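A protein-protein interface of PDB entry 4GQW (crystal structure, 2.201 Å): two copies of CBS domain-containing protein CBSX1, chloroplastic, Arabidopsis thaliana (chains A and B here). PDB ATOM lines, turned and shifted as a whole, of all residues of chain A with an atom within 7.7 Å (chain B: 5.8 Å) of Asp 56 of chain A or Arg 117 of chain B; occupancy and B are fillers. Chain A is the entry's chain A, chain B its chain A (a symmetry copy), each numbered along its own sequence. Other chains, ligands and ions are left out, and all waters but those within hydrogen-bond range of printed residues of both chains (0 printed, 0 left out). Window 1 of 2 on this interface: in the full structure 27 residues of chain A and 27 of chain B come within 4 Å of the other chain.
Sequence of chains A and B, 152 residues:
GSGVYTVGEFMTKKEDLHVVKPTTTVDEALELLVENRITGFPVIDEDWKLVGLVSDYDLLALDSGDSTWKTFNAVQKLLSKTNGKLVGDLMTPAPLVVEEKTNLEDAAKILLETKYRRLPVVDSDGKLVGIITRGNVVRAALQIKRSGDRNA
OD2 of Asp 56 of chain A is in salt-bridge range of NE of Arg 117 of chain B (3.0 Å).
NH1 of Arg 134 of chain B is in salt-bridge range of OD1 of Asp 56 of chain A, 3.6 Å away.
Among the printed residues, pairs that only touch across the chains: Tyr 57 of chain A with Arg 117 of chain B and Leu 62 of chain A with Arg 134 of chain B.
The backbone NH (N) of Asp 56 of chain A is in hydrogen-bond range of the backbone carbonyl oxygen (O) of Thr 39 of chain A (2.9 Å).
The backbone carbonyl oxygen (O) of Tyr 57 of chain A sits at hydrogen-bond distance from the backbone NH (N) of Leu 62 of chain A, 3.1 Å away.
O of Leu 111 of chain B sits at hydrogen-bond distance from NE of Arg 134 of chain B.
The backbone carbonyl oxygen of Tyr 116 of chain B sits at hydrogen-bond distance from the guanidinium group of Arg 134 of chain B (3.0 Å).
N of Arg 134 of chain B sits at hydrogen-bond distance from O of Arg 117 of chain B (2.9 Å).
2 positions are printed for both chains.
Of the 20 printed residues of chain A, 3 touch a printed residue of chain B.
Of the 10 printed residues of chain B, 2 touch a printed residue of chain A.
Printed residues of chain B that touch a printed residue of chain A: Arg 117 and Arg 134.
Among the printed residues, 4 pairs touch across the chains.
Of chain B, only Arg 117 and Arg 134 come within 4 Å of Asp 56 of chain A.
Printed residues of chain A within 4 Å of Arg 117 of chain B: Asp 56 and Tyr 57.
Of the printed residues of chain A, Arg 134 of chain B touches Asp 56 and Leu 62.
Of the printed residues of chain B, Leu 62 of chain A touches Arg 134 (3.8 Å).
Lys 115 of chain B touches none of the printed residues of chain A.
The nearest residue of chain A that does not touch Arg 117 of chain B is Thr 39 of chain A (4.3 Å).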
ATOM      1  N   VAL A  26     -22.243  15.239  -0.409  1.00  0.00           N
ATOM      2  CA  VAL A  26     -22.558  13.920   0.121  1.00  0.00           C
ATOM      3  C   VAL A  26     -23.437  14.044   1.357  1.00  0.00           C
ATOM      4  O   VAL A  26     -24.311  13.215   1.596  1.00  0.00           O
ATOM      5  CB  VAL A  26     -21.270  13.153   0.476  1.00  0.00           C
ATOM      6  CG1 VAL A  26     -21.596  11.775   1.024  1.00  0.00           C
ATOM      7  CG2 VAL A  26     -20.377  13.043  -0.748  1.00  0.00           C
ATOM      8  N   LEU A  30     -27.057  12.322   1.764  1.00  0.00           N
ATOM      9  CA  LEU A  30     -27.355  11.369   2.825  1.00  0.00           C
ATOM     10  C   LEU A  30     -28.591  11.798   3.603  1.00  0.00           C
ATOM     11  O   LEU A  30     -29.446  10.973   3.933  1.00  0.00           O
ATOM     12  CB  LEU A  30     -26.165  11.225   3.774  1.00  0.00           C
ATOM     13  CG  LEU A  30     -24.920  10.530   3.219  1.00  0.00           C
ATOM     14  CD1 LEU A  30     -23.814  10.512   4.263  1.00  0.00           C
ATOM     15  CD2 LEU A  30     -25.253   9.118   2.764  1.00  0.00           C
ATOM     16  N   LEU A  33     -31.579  11.036   1.636  1.00  0.00           N
ATOM     17  CA  LEU A  33     -31.793   9.596   1.740  1.00  0.00           C
ATOM     18  C   LEU A  33     -32.563   9.255   3.006  1.00  0.00           C
ATOM     19  O   LEU A  33     -33.536   8.504   2.969  1.00  0.00           O
ATOM     20  CB  LEU A  33     -30.458   8.851   1.761  1.00  0.00           C
ATOM     21  CG  LEU A  33     -29.668   8.726   0.461  1.00  0.00           C
ATOM     22  CD1 LEU A  33     -28.323   8.069   0.721  1.00  0.00           C
ATOM     23  CD2 LEU A  33     -30.464   7.930  -0.548  1.00  0.00           C
ATOM     24  N   ILE A  38     -34.984   6.388   1.268  1.00  0.00           N
ATOM     25  CA  ILE A  38     -34.522   5.820   0.004  1.00  0.00           C
ATOM     26  C   ILE A  38     -33.071   5.357   0.057  1.00  0.00           C
ATOM     27  O   ILE A  38     -32.350   5.654   1.008  1.00  0.00           O
ATOM     28  CB  ILE A  38     -34.690   6.814  -1.151  1.00  0.00           C
ATOM     29  CG1 ILE A  38     -34.272   8.214  -0.699  1.00  0.00           C
ATOM     30  CG2 ILE A  38     -36.131   6.821  -1.634  1.00  0.00           C
ATOM     31  CD1 ILE A  38     -34.522   9.290  -1.727  1.00  0.00           C
ATOM     32  N   THR A  39     -32.651   4.635  -0.977  1.00  0.00           N
ATOM     33  CA  THR A  39     -31.302   4.085  -1.032  1.00  0.00           C
ATOM     34  C   THR A  39     -30.449   4.771  -2.095  1.00  0.00           C
ATOM     35  O   THR A  39     -29.253   4.505  -2.207  1.00  0.00           O
ATOM     36  CB  THR A  39     -31.325   2.580  -1.325  1.00  0.00           C
ATOM     37  OG1 THR A  39     -31.731   2.359  -2.682  1.00  0.00           O
ATOM     38  CG2 THR A  39     -32.293   1.877  -0.390  1.00  0.00           C
ATOM     39  N   GLY A  40     -31.069   5.647  -2.879  1.00  0.00           N
ATOM     40  CA  GLY A  40     -30.350   6.382  -3.902  1.00  0.00           C
ATOM     41  C   GLY A  40     -31.236   7.288  -4.731  1.00  0.00           C
ATOM     42  O   GLY A  40     -32.459   7.253  -4.613  1.00  0.00           O
ATOM     43  N   PHE A  41     -30.610   8.107  -5.570  1.00  0.00           N
ATOM     44  CA  PHE A  41     -31.341   8.969  -6.489  1.00  0.00           C
ATOM     45  C   PHE A  41     -30.710   8.976  -7.867  1.00  0.00           C
ATOM     46  O   PHE A  41     -29.551   8.593  -8.036  1.00  0.00           O
ATOM     47  CB  PHE A  41     -31.378  10.423  -6.008  1.00  0.00           C
ATOM     48  CG  PHE A  41     -30.886  10.628  -4.615  1.00  0.00           C
ATOM     49  CD1 PHE A  41     -31.784  10.780  -3.577  1.00  0.00           C
ATOM     50  CD2 PHE A  41     -29.530  10.717  -4.347  1.00  0.00           C
ATOM     51  CE1 PHE A  41     -31.344  10.992  -2.297  1.00  0.00           C
ATOM     52  CE2 PHE A  41     -29.084  10.924  -3.066  1.00  0.00           C
ATOM     53  CZ  PHE A  41     -29.992  11.065  -2.041  1.00  0.00           C
ATOM     54  N   VAL A  54     -26.780   7.716  -8.261  1.00  0.00           N
ATOM     55  CA  VAL A  54     -25.968   7.632  -7.057  1.00  0.00           C
ATOM     56  C   VAL A  54     -26.708   6.921  -5.933  1.00  0.00           C
ATOM     57  O   VAL A  54     -27.897   7.143  -5.722  1.00  0.00           O
ATOM     58  CB  VAL A  54     -25.455   9.022  -6.606  1.00  0.00           C
ATOM     59  CG1 VAL A  54     -26.602   9.928  -6.202  1.00  0.00           C
ATOM     60  CG2 VAL A  54     -24.457   8.878  -5.473  1.00  0.00           C
ATOM     61  N   SER A  55     -26.001   6.044  -5.231  1.00  0.00           N
ATOM     62  CA  SER A  55     -26.601   5.282  -4.146  1.00  0.00           C
ATOM     63  C   SER A  55     -25.843   5.480  -2.843  1.00  0.00           C
ATOM     64  O   SER A  55     -24.817   6.158  -2.802  1.00  0.00           O
ATOM     65  CB  SER A  55     -26.642   3.796  -4.501  1.00  0.00           C
ATOM     66  OG  SER A  55     -27.441   3.579  -5.650  1.00  0.00           O
ATOM     67  N   ASP A  56     -26.358   4.874  -1.779  1.00  0.00           N
ATOM     68  CA  ASP A  56     -25.757   4.987  -0.455  1.00  0.00           C
ATOM     69  C   ASP A  56     -24.336   4.432  -0.387  1.00  0.00           C
ATOM     70  O   ASP A  56     -23.471   5.016   0.264  1.00  0.00           O
ATOM     71  CB  ASP A  56     -26.647   4.317   0.595  1.00  0.00           C
ATOM     72  CG  ASP A  56     -27.075   2.919   0.195  1.00  0.00           C
ATOM     73  OD1 ASP A  56     -26.361   2.272  -0.598  1.00  0.00           O
ATOM     74  OD2 ASP A  56     -28.129   2.461   0.682  1.00  0.00           O
ATOM     75  N   TYR A  57     -24.089   3.314  -1.061  1.00  0.00           N
ATOM     76  CA  TYR A  57     -22.754   2.722  -1.045  1.00  0.00           C
ATOM     77  C   TYR A  57     -21.747   3.586  -1.800  1.00  0.00           C
ATOM     78  O   TYR A  57     -20.558   3.580  -1.489  1.00  0.00           O
ATOM     79  CB  TYR A  57     -22.764   1.286  -1.580  1.00  0.00           C
ATOM     80  CG  TYR A  57     -23.383   1.120  -2.947  1.00  0.00           C
ATOM     81  CD1 TYR A  57     -22.639   1.320  -4.099  1.00  0.00           C
ATOM     82  CD2 TYR A  57     -24.711   0.748  -3.083  1.00  0.00           C
ATOM     83  CE1 TYR A  57     -23.203   1.163  -5.351  1.00  0.00           C
ATOM     84  CE2 TYR A  57     -25.284   0.587  -4.330  1.00  0.00           C
ATOM     85  CZ  TYR A  57     -24.526   0.798  -5.460  1.00  0.00           C
ATOM     86  OH  TYR A  57     -25.097   0.639  -6.701  1.00  0.00           O
ATOM     87  N   ASP A  58     -22.230   4.332  -2.788  1.00  0.00           N
ATOM     88  CA  ASP A  58     -21.385   5.276  -3.504  1.00  0.00           C
ATOM     89  C   ASP A  58     -21.025   6.445  -2.597  1.00  0.00           C
ATOM     90  O   ASP A  58     -19.874   6.875  -2.547  1.00  0.00           O
ATOM     91  CB  ASP A  58     -22.095   5.799  -4.754  1.00  0.00           C
ATOM     92  CG  ASP A  58     -22.306   4.726  -5.794  1.00  0.00           C
ATOM     93  OD1 ASP A  58     -21.387   3.908  -5.999  1.00  0.00           O
ATOM     94  OD2 ASP A  58     -23.392   4.701  -6.408  1.00  0.00           O
ATOM     95  N   LEU A  59     -22.019   6.949  -1.875  1.00  0.00           N
ATOM     96  CA  LEU A  59     -21.843   8.125  -1.032  1.00  0.00           C
ATOM     97  C   LEU A  59     -20.983   7.846   0.193  1.00  0.00           C
ATOM     98  O   LEU A  59     -20.204   8.697   0.616  1.00  0.00           O
ATOM     99  CB  LEU A  59     -23.204   8.664  -0.600  1.00  0.00           C
ATOM    100  CG  LEU A  59     -24.073   9.189  -1.741  1.00  0.00           C
ATOM    101  CD1 LEU A  59     -25.487   9.435  -1.254  1.00  0.00           C
ATOM    102  CD2 LEU A  59     -23.472  10.466  -2.303  1.00  0.00           C
ATOM    103  N   LEU A  60     -21.126   6.656   0.763  1.00  0.00           N
ATOM    104  CA  LEU A  60     -20.353   6.297   1.942  1.00  0.00           C
ATOM    105  C   LEU A  60     -19.030   5.667   1.535  1.00  0.00           C
ATOM    106  O   LEU A  60     -18.184   5.382   2.383  1.00  0.00           O
ATOM    107  CB  LEU A  60     -21.145   5.335   2.824  1.00  0.00           C
ATOM    108  CG  LEU A  60     -22.522   5.826   3.274  1.00  0.00           C
ATOM    109  CD1 LEU A  60     -23.270   4.711   3.982  1.00  0.00           C
ATOM    110  CD2 LEU A  60     -22.380   7.031   4.181  1.00  0.00           C
ATOM    111  N   ALA A  61     -18.868   5.464   0.229  1.00  0.00           N
ATOM    112  CA  ALA A  61     -17.657   4.878  -0.339  1.00  0.00           C
ATOM    113  C   ALA A  61     -17.306   3.537   0.296  1.00  0.00           C
ATOM    114  O   ALA A  61     -16.239   3.383   0.889  1.00  0.00           O
ATOM    115  CB  ALA A  61     -16.486   5.847  -0.218  1.00  0.00           C
ATOM    116  N   LEU A  62     -18.206   2.568   0.170  1.00  0.00           N
ATOM    117  CA  LEU A  62     -17.988   1.254   0.762  1.00  0.00           C
ATOM    118  C   LEU A  62     -17.147   0.372  -0.143  1.00  0.00           C
ATOM    119  O   LEU A  62     -16.404  -0.487   0.328  1.00  0.00           O
ATOM    120  CB  LEU A  62     -19.321   0.570   1.040  1.00  0.00           C
ATOM    121  CG  LEU A  62     -20.311   1.428   1.820  1.00  0.00           C
ATOM    122  CD1 LEU A  62     -21.585   0.646   2.084  1.00  0.00           C
ATOM    123  CD2 LEU A  62     -19.677   1.894   3.115  1.00  0.00           C
ATOM    124  N   ASP A  63     -17.270   0.583  -1.448  1.00  0.00           N
ATOM    125  CA  ASP A  63     -16.519  -0.210  -2.412  1.00  0.00           C
ATOM    126  C   ASP A  63     -15.192   0.459  -2.754  1.00  0.00           C
ATOM    127  O   ASP A  63     -14.421   0.818  -1.864  1.00  0.00           O
ATOM    128  CB  ASP A  63     -17.350  -0.448  -3.675  1.00  0.00           C
ATOM    129  CG  ASP A  63     -18.661  -1.152  -3.385  1.00  0.00           C
ATOM    130  OD1 ASP A  63     -19.209  -0.955  -2.280  1.00  0.00           O
ATOM    131  OD2 ASP A  63     -19.148  -1.900  -4.259  1.00  0.00           O
ATOM    132  N   LEU A  90     -18.847  10.728  -7.244  1.00  0.00           N
ATOM    133  CA  LEU A  90     -19.188   9.429  -6.683  1.00  0.00           C
ATOM    134  C   LEU A  90     -20.272   8.711  -7.479  1.00  0.00           C
ATOM    135  O   LEU A  90     -20.388   7.489  -7.416  1.00  0.00           O
ATOM    136  CB  LEU A  90     -19.629   9.578  -5.226  1.00  0.00           C
ATOM    137  CG  LEU A  90     -18.573  10.103  -4.253  1.00  0.00           C
ATOM    138  CD1 LEU A  90     -19.165  10.259  -2.863  1.00  0.00           C
ATOM    139  CD2 LEU A  90     -17.377   9.173  -4.221  1.00  0.00           C
ATOM    140  N   ARG A 117     -33.230  -2.942  -9.948  1.00  0.00           N
ATOM    141  CA  ARG A 117     -34.557  -2.702  -9.400  1.00  0.00           C
ATOM    142  C   ARG A 117     -35.139  -1.400  -9.924  1.00  0.00           C
ATOM    143  O   ARG A 117     -36.353  -1.215  -9.918  1.00  0.00           O
ATOM    144  CB  ARG A 117     -34.518  -2.659  -7.872  1.00  0.00           C
ATOM    145  CG  ARG A 117     -34.439  -4.016  -7.207  1.00  0.00           C
ATOM    146  CD  ARG A 117     -34.735  -3.888  -5.722  1.00  0.00           C
ATOM    147  NE  ARG A 117     -34.785  -5.186  -5.062  1.00  0.00           N
ATOM    148  CZ  ARG A 117     -33.909  -5.594  -4.151  1.00  0.00           C
ATOM    149  NH1 ARG A 117     -32.916  -4.798  -3.780  1.00  0.00           N
ATOM    150  NH2 ARG A 117     -34.032  -6.794  -3.604  1.00  0.00           N
ATOM    151  N   ARG A 118     -34.273  -0.495 -10.367  1.00  0.00           N
ATOM    152  CA  ARG A 118     -34.719   0.828 -10.790  1.00  0.00           C
ATOM    153  C   ARG A 118     -34.185   1.214 -12.162  1.00  0.00           C
ATOM    154  O   ARG A 118     -32.988   1.113 -12.426  1.00  0.00           O
ATOM    155  CB  ARG A 118     -34.290   1.887  -9.774  1.00  0.00           C
ATOM    156  CG  ARG A 118     -34.637   1.554  -8.335  1.00  0.00           C
ATOM    157  CD  ARG A 118     -34.297   2.710  -7.414  1.00  0.00           C
ATOM    158  NE  ARG A 118     -33.304   2.342  -6.408  1.00  0.00           N
ATOM    159  CZ  ARG A 118     -32.286   3.117  -6.049  1.00  0.00           C
ATOM    160  NH1 ARG A 118     -32.123   4.304  -6.616  1.00  0.00           N
ATOM    161  NH2 ARG A 118     -31.429   2.707  -5.125  1.00  0.00           N
ATOM    162  N   LEU B 111     -23.122  -3.345   8.500  1.00  0.00           N
ATOM    163  CA  LEU B 111     -23.907  -2.689   7.463  1.00  0.00           C
ATOM    164  C   LEU B 111     -23.066  -1.824   6.536  1.00  0.00           C
ATOM    165  O   LEU B 111     -23.595  -1.206   5.615  1.00  0.00           O
ATOM    166  CB  LEU B 111     -25.000  -1.837   8.101  1.00  0.00           C
ATOM    167  CG  LEU B 111     -26.024  -2.606   8.936  1.00  0.00           C
ATOM    168  CD1 LEU B 111     -26.813  -1.659   9.826  1.00  0.00           C
ATOM    169  CD2 LEU B 111     -26.946  -3.399   8.033  1.00  0.00           C
ATOM    170  N   LYS B 115     -22.569  -6.385   2.299  1.00  0.00           N
ATOM    171  CA  LYS B 115     -23.576  -5.982   1.331  1.00  0.00           C
ATOM    172  C   LYS B 115     -24.965  -5.987   1.959  1.00  0.00           C
ATOM    173  O   LYS B 115     -25.965  -5.776   1.274  1.00  0.00           O
ATOM    174  CB  LYS B 115     -23.542  -6.910   0.114  1.00  0.00           C
ATOM    175  CG  LYS B 115     -22.255  -6.824  -0.694  1.00  0.00           C
ATOM    176  CD  LYS B 115     -22.131  -7.973  -1.689  1.00  0.00           C
ATOM    177  CE  LYS B 115     -20.868  -7.833  -2.531  1.00  0.00           C
ATOM    178  NZ  LYS B 115     -20.704  -8.980  -3.465  1.00  0.00           N
ATOM    179  N   TYR B 116     -25.027  -6.230   3.264  1.00  0.00           N
ATOM    180  CA  TYR B 116     -26.304  -6.219   3.967  1.00  0.00           C
ATOM    181  C   TYR B 116     -26.743  -4.793   4.269  1.00  0.00           C
ATOM    182  O   TYR B 116     -25.975  -3.998   4.807  1.00  0.00           O
ATOM    183  CB  TYR B 116     -26.228  -7.023   5.268  1.00  0.00           C
ATOM    184  CG  TYR B 116     -25.863  -8.475   5.076  1.00  0.00           C
ATOM    185  CD1 TYR B 116     -26.819  -9.413   4.720  1.00  0.00           C
ATOM    186  CD2 TYR B 116     -24.560  -8.910   5.258  1.00  0.00           C
ATOM    187  CE1 TYR B 116     -26.483 -10.743   4.546  1.00  0.00           C
ATOM    188  CE2 TYR B 116     -24.216 -10.233   5.086  1.00  0.00           C
ATOM    189  CZ  TYR B 116     -25.179 -11.145   4.730  1.00  0.00           C
ATOM    190  OH  TYR B 116     -24.838 -12.464   4.557  1.00  0.00           O
ATOM    191  N   ARG B 117     -27.980  -4.472   3.913  1.00  0.00           N
ATOM    192  CA  ARG B 117     -28.553  -3.178   4.254  1.00  0.00           C
ATOM    193  C   ARG B 117     -29.454  -3.281   5.472  1.00  0.00           C
ATOM    194  O   ARG B 117     -29.701  -2.288   6.149  1.00  0.00           O
ATOM    195  CB  ARG B 117     -29.352  -2.608   3.082  1.00  0.00           C
ATOM    196  CG  ARG B 117     -28.507  -1.996   1.984  1.00  0.00           C
ATOM    197  CD  ARG B 117     -29.380  -1.180   1.047  1.00  0.00           C
ATOM    198  NE  ARG B 117     -28.593  -0.477   0.042  1.00  0.00           N
ATOM    199  CZ  ARG B 117     -28.637  -0.741  -1.259  1.00  0.00           C
ATOM    200  NH1 ARG B 117     -29.442  -1.690  -1.718  1.00  0.00           N
ATOM    201  NH2 ARG B 117     -27.883  -0.051  -2.102  1.00  0.00           N
ATOM    202  N   ARG B 118     -29.955  -4.483   5.744  1.00  0.00           N
ATOM    203  CA  ARG B 118     -30.916  -4.669   6.825  1.00  0.00           C
ATOM    204  C   ARG B 118     -30.526  -5.801   7.765  1.00  0.00           C
ATOM    205  O   ARG B 118     -30.224  -6.911   7.328  1.00  0.00           O
ATOM    206  CB  ARG B 118     -32.308  -4.950   6.261  1.00  0.00           C
ATOM    207  CG  ARG B 118     -32.765  -3.968   5.198  1.00  0.00           C
ATOM    208  CD  ARG B 118     -34.200  -4.240   4.788  1.00  0.00           C
ATOM    209  NE  ARG B 118     -34.316  -4.579   3.373  1.00  0.00           N
ATOM    210  CZ  ARG B 118     -35.095  -5.547   2.901  1.00  0.00           C
ATOM    211  NH1 ARG B 118     -35.825  -6.277   3.734  1.00  0.00           N
ATOM    212  NH2 ARG B 118     -35.144  -5.790   1.600  1.00  0.00           N
ATOM    213  N   LEU B 119     -30.553  -5.514   9.060  1.00  0.00           N
ATOM    214  CA  LEU B 119     -30.315  -6.526  10.078  1.00  0.00           C
ATOM    215  C   LEU B 119     -31.479  -6.587  11.055  1.00  0.00           C
ATOM    216  O   LEU B 119     -31.841  -5.582  11.655  1.00  0.00           O
ATOM    217  CB  LEU B 119     -29.026  -6.230  10.845  1.00  0.00           C
ATOM    218  CG  LEU B 119     -27.699  -6.413  10.110  1.00  0.00           C
ATOM    219  CD1 LEU B 119     -26.552  -6.104  11.053  1.00  0.00           C
ATOM    220  CD2 LEU B 119     -27.589  -7.826   9.578  1.00  0.00           C
ATOM    221  N   ILE B 132     -32.712  -2.870  12.134  1.00  0.00           N
ATOM    222  CA  ILE B 132     -31.729  -1.808  11.954  1.00  0.00           C
ATOM    223  C   ILE B 132     -31.215  -1.785  10.516  1.00  0.00           C
ATOM    224  O   ILE B 132     -30.727  -2.791  10.000  1.00  0.00           O
ATOM    225  CB  ILE B 132     -30.549  -1.934  12.953  1.00  0.00           C
ATOM    226  CG1 ILE B 132     -29.476  -0.883  12.656  1.00  0.00           C
ATOM    227  CG2 ILE B 132     -29.963  -3.335  12.949  1.00  0.00           C
ATOM    228  CD1 ILE B 132     -29.759   0.452  13.293  1.00  0.00           C
ATOM    229  N   THR B 133     -31.342  -0.636   9.861  1.00  0.00           N
ATOM    230  CA  THR B 133     -30.930  -0.520   8.468  1.00  0.00           C
ATOM    231  C   THR B 133     -29.718   0.385   8.303  1.00  0.00           C
ATOM    232  O   THR B 133     -29.289   1.047   9.245  1.00  0.00           O
ATOM    233  CB  THR B 133     -32.070   0.002   7.570  1.00  0.00           C
ATOM    234  OG1 THR B 133     -32.378   1.357   7.918  1.00  0.00           O
ATOM    235  CG2 THR B 133     -33.310  -0.856   7.731  1.00  0.00           C
ATOM    236  N   ARG B 134     -29.170   0.398   7.096  1.00  0.00           N
ATOM    237  CA  ARG B 134     -28.042   1.255   6.774  1.00  0.00           C
ATOM    238  C   ARG B 134     -28.456   2.713   6.897  1.00  0.00           C
ATOM    239  O   ARG B 134     -27.693   3.558   7.375  1.00  0.00           O
ATOM    240  CB  ARG B 134     -27.567   0.963   5.356  1.00  0.00           C
ATOM    241  CG  ARG B 134     -26.312   1.698   4.971  1.00  0.00           C
ATOM    242  CD  ARG B 134     -25.799   1.193   3.646  1.00  0.00           C
ATOM    243  NE  ARG B 134     -25.361  -0.196   3.732  1.00  0.00           N
ATOM    244  CZ  ARG B 134     -25.066  -0.946   2.678  1.00  0.00           C
ATOM    245  NH1 ARG B 134     -25.171  -0.440   1.457  1.00  0.00           N
ATOM    246  NH2 ARG B 134     -24.672  -2.201   2.840  1.00  0.00           N
ATOM    247  N   GLY B 135     -29.682   2.994   6.467  1.00  0.00           N
ATOM    248  CA  GLY B 135     -30.244   4.325   6.567  1.00  0.00           C
ATOM    249  C   GLY B 135     -30.398   4.748   8.009  1.00  0.00           C
ATOM    250  O   GLY B 135     -30.248   5.923   8.332  1.00  0.00           O
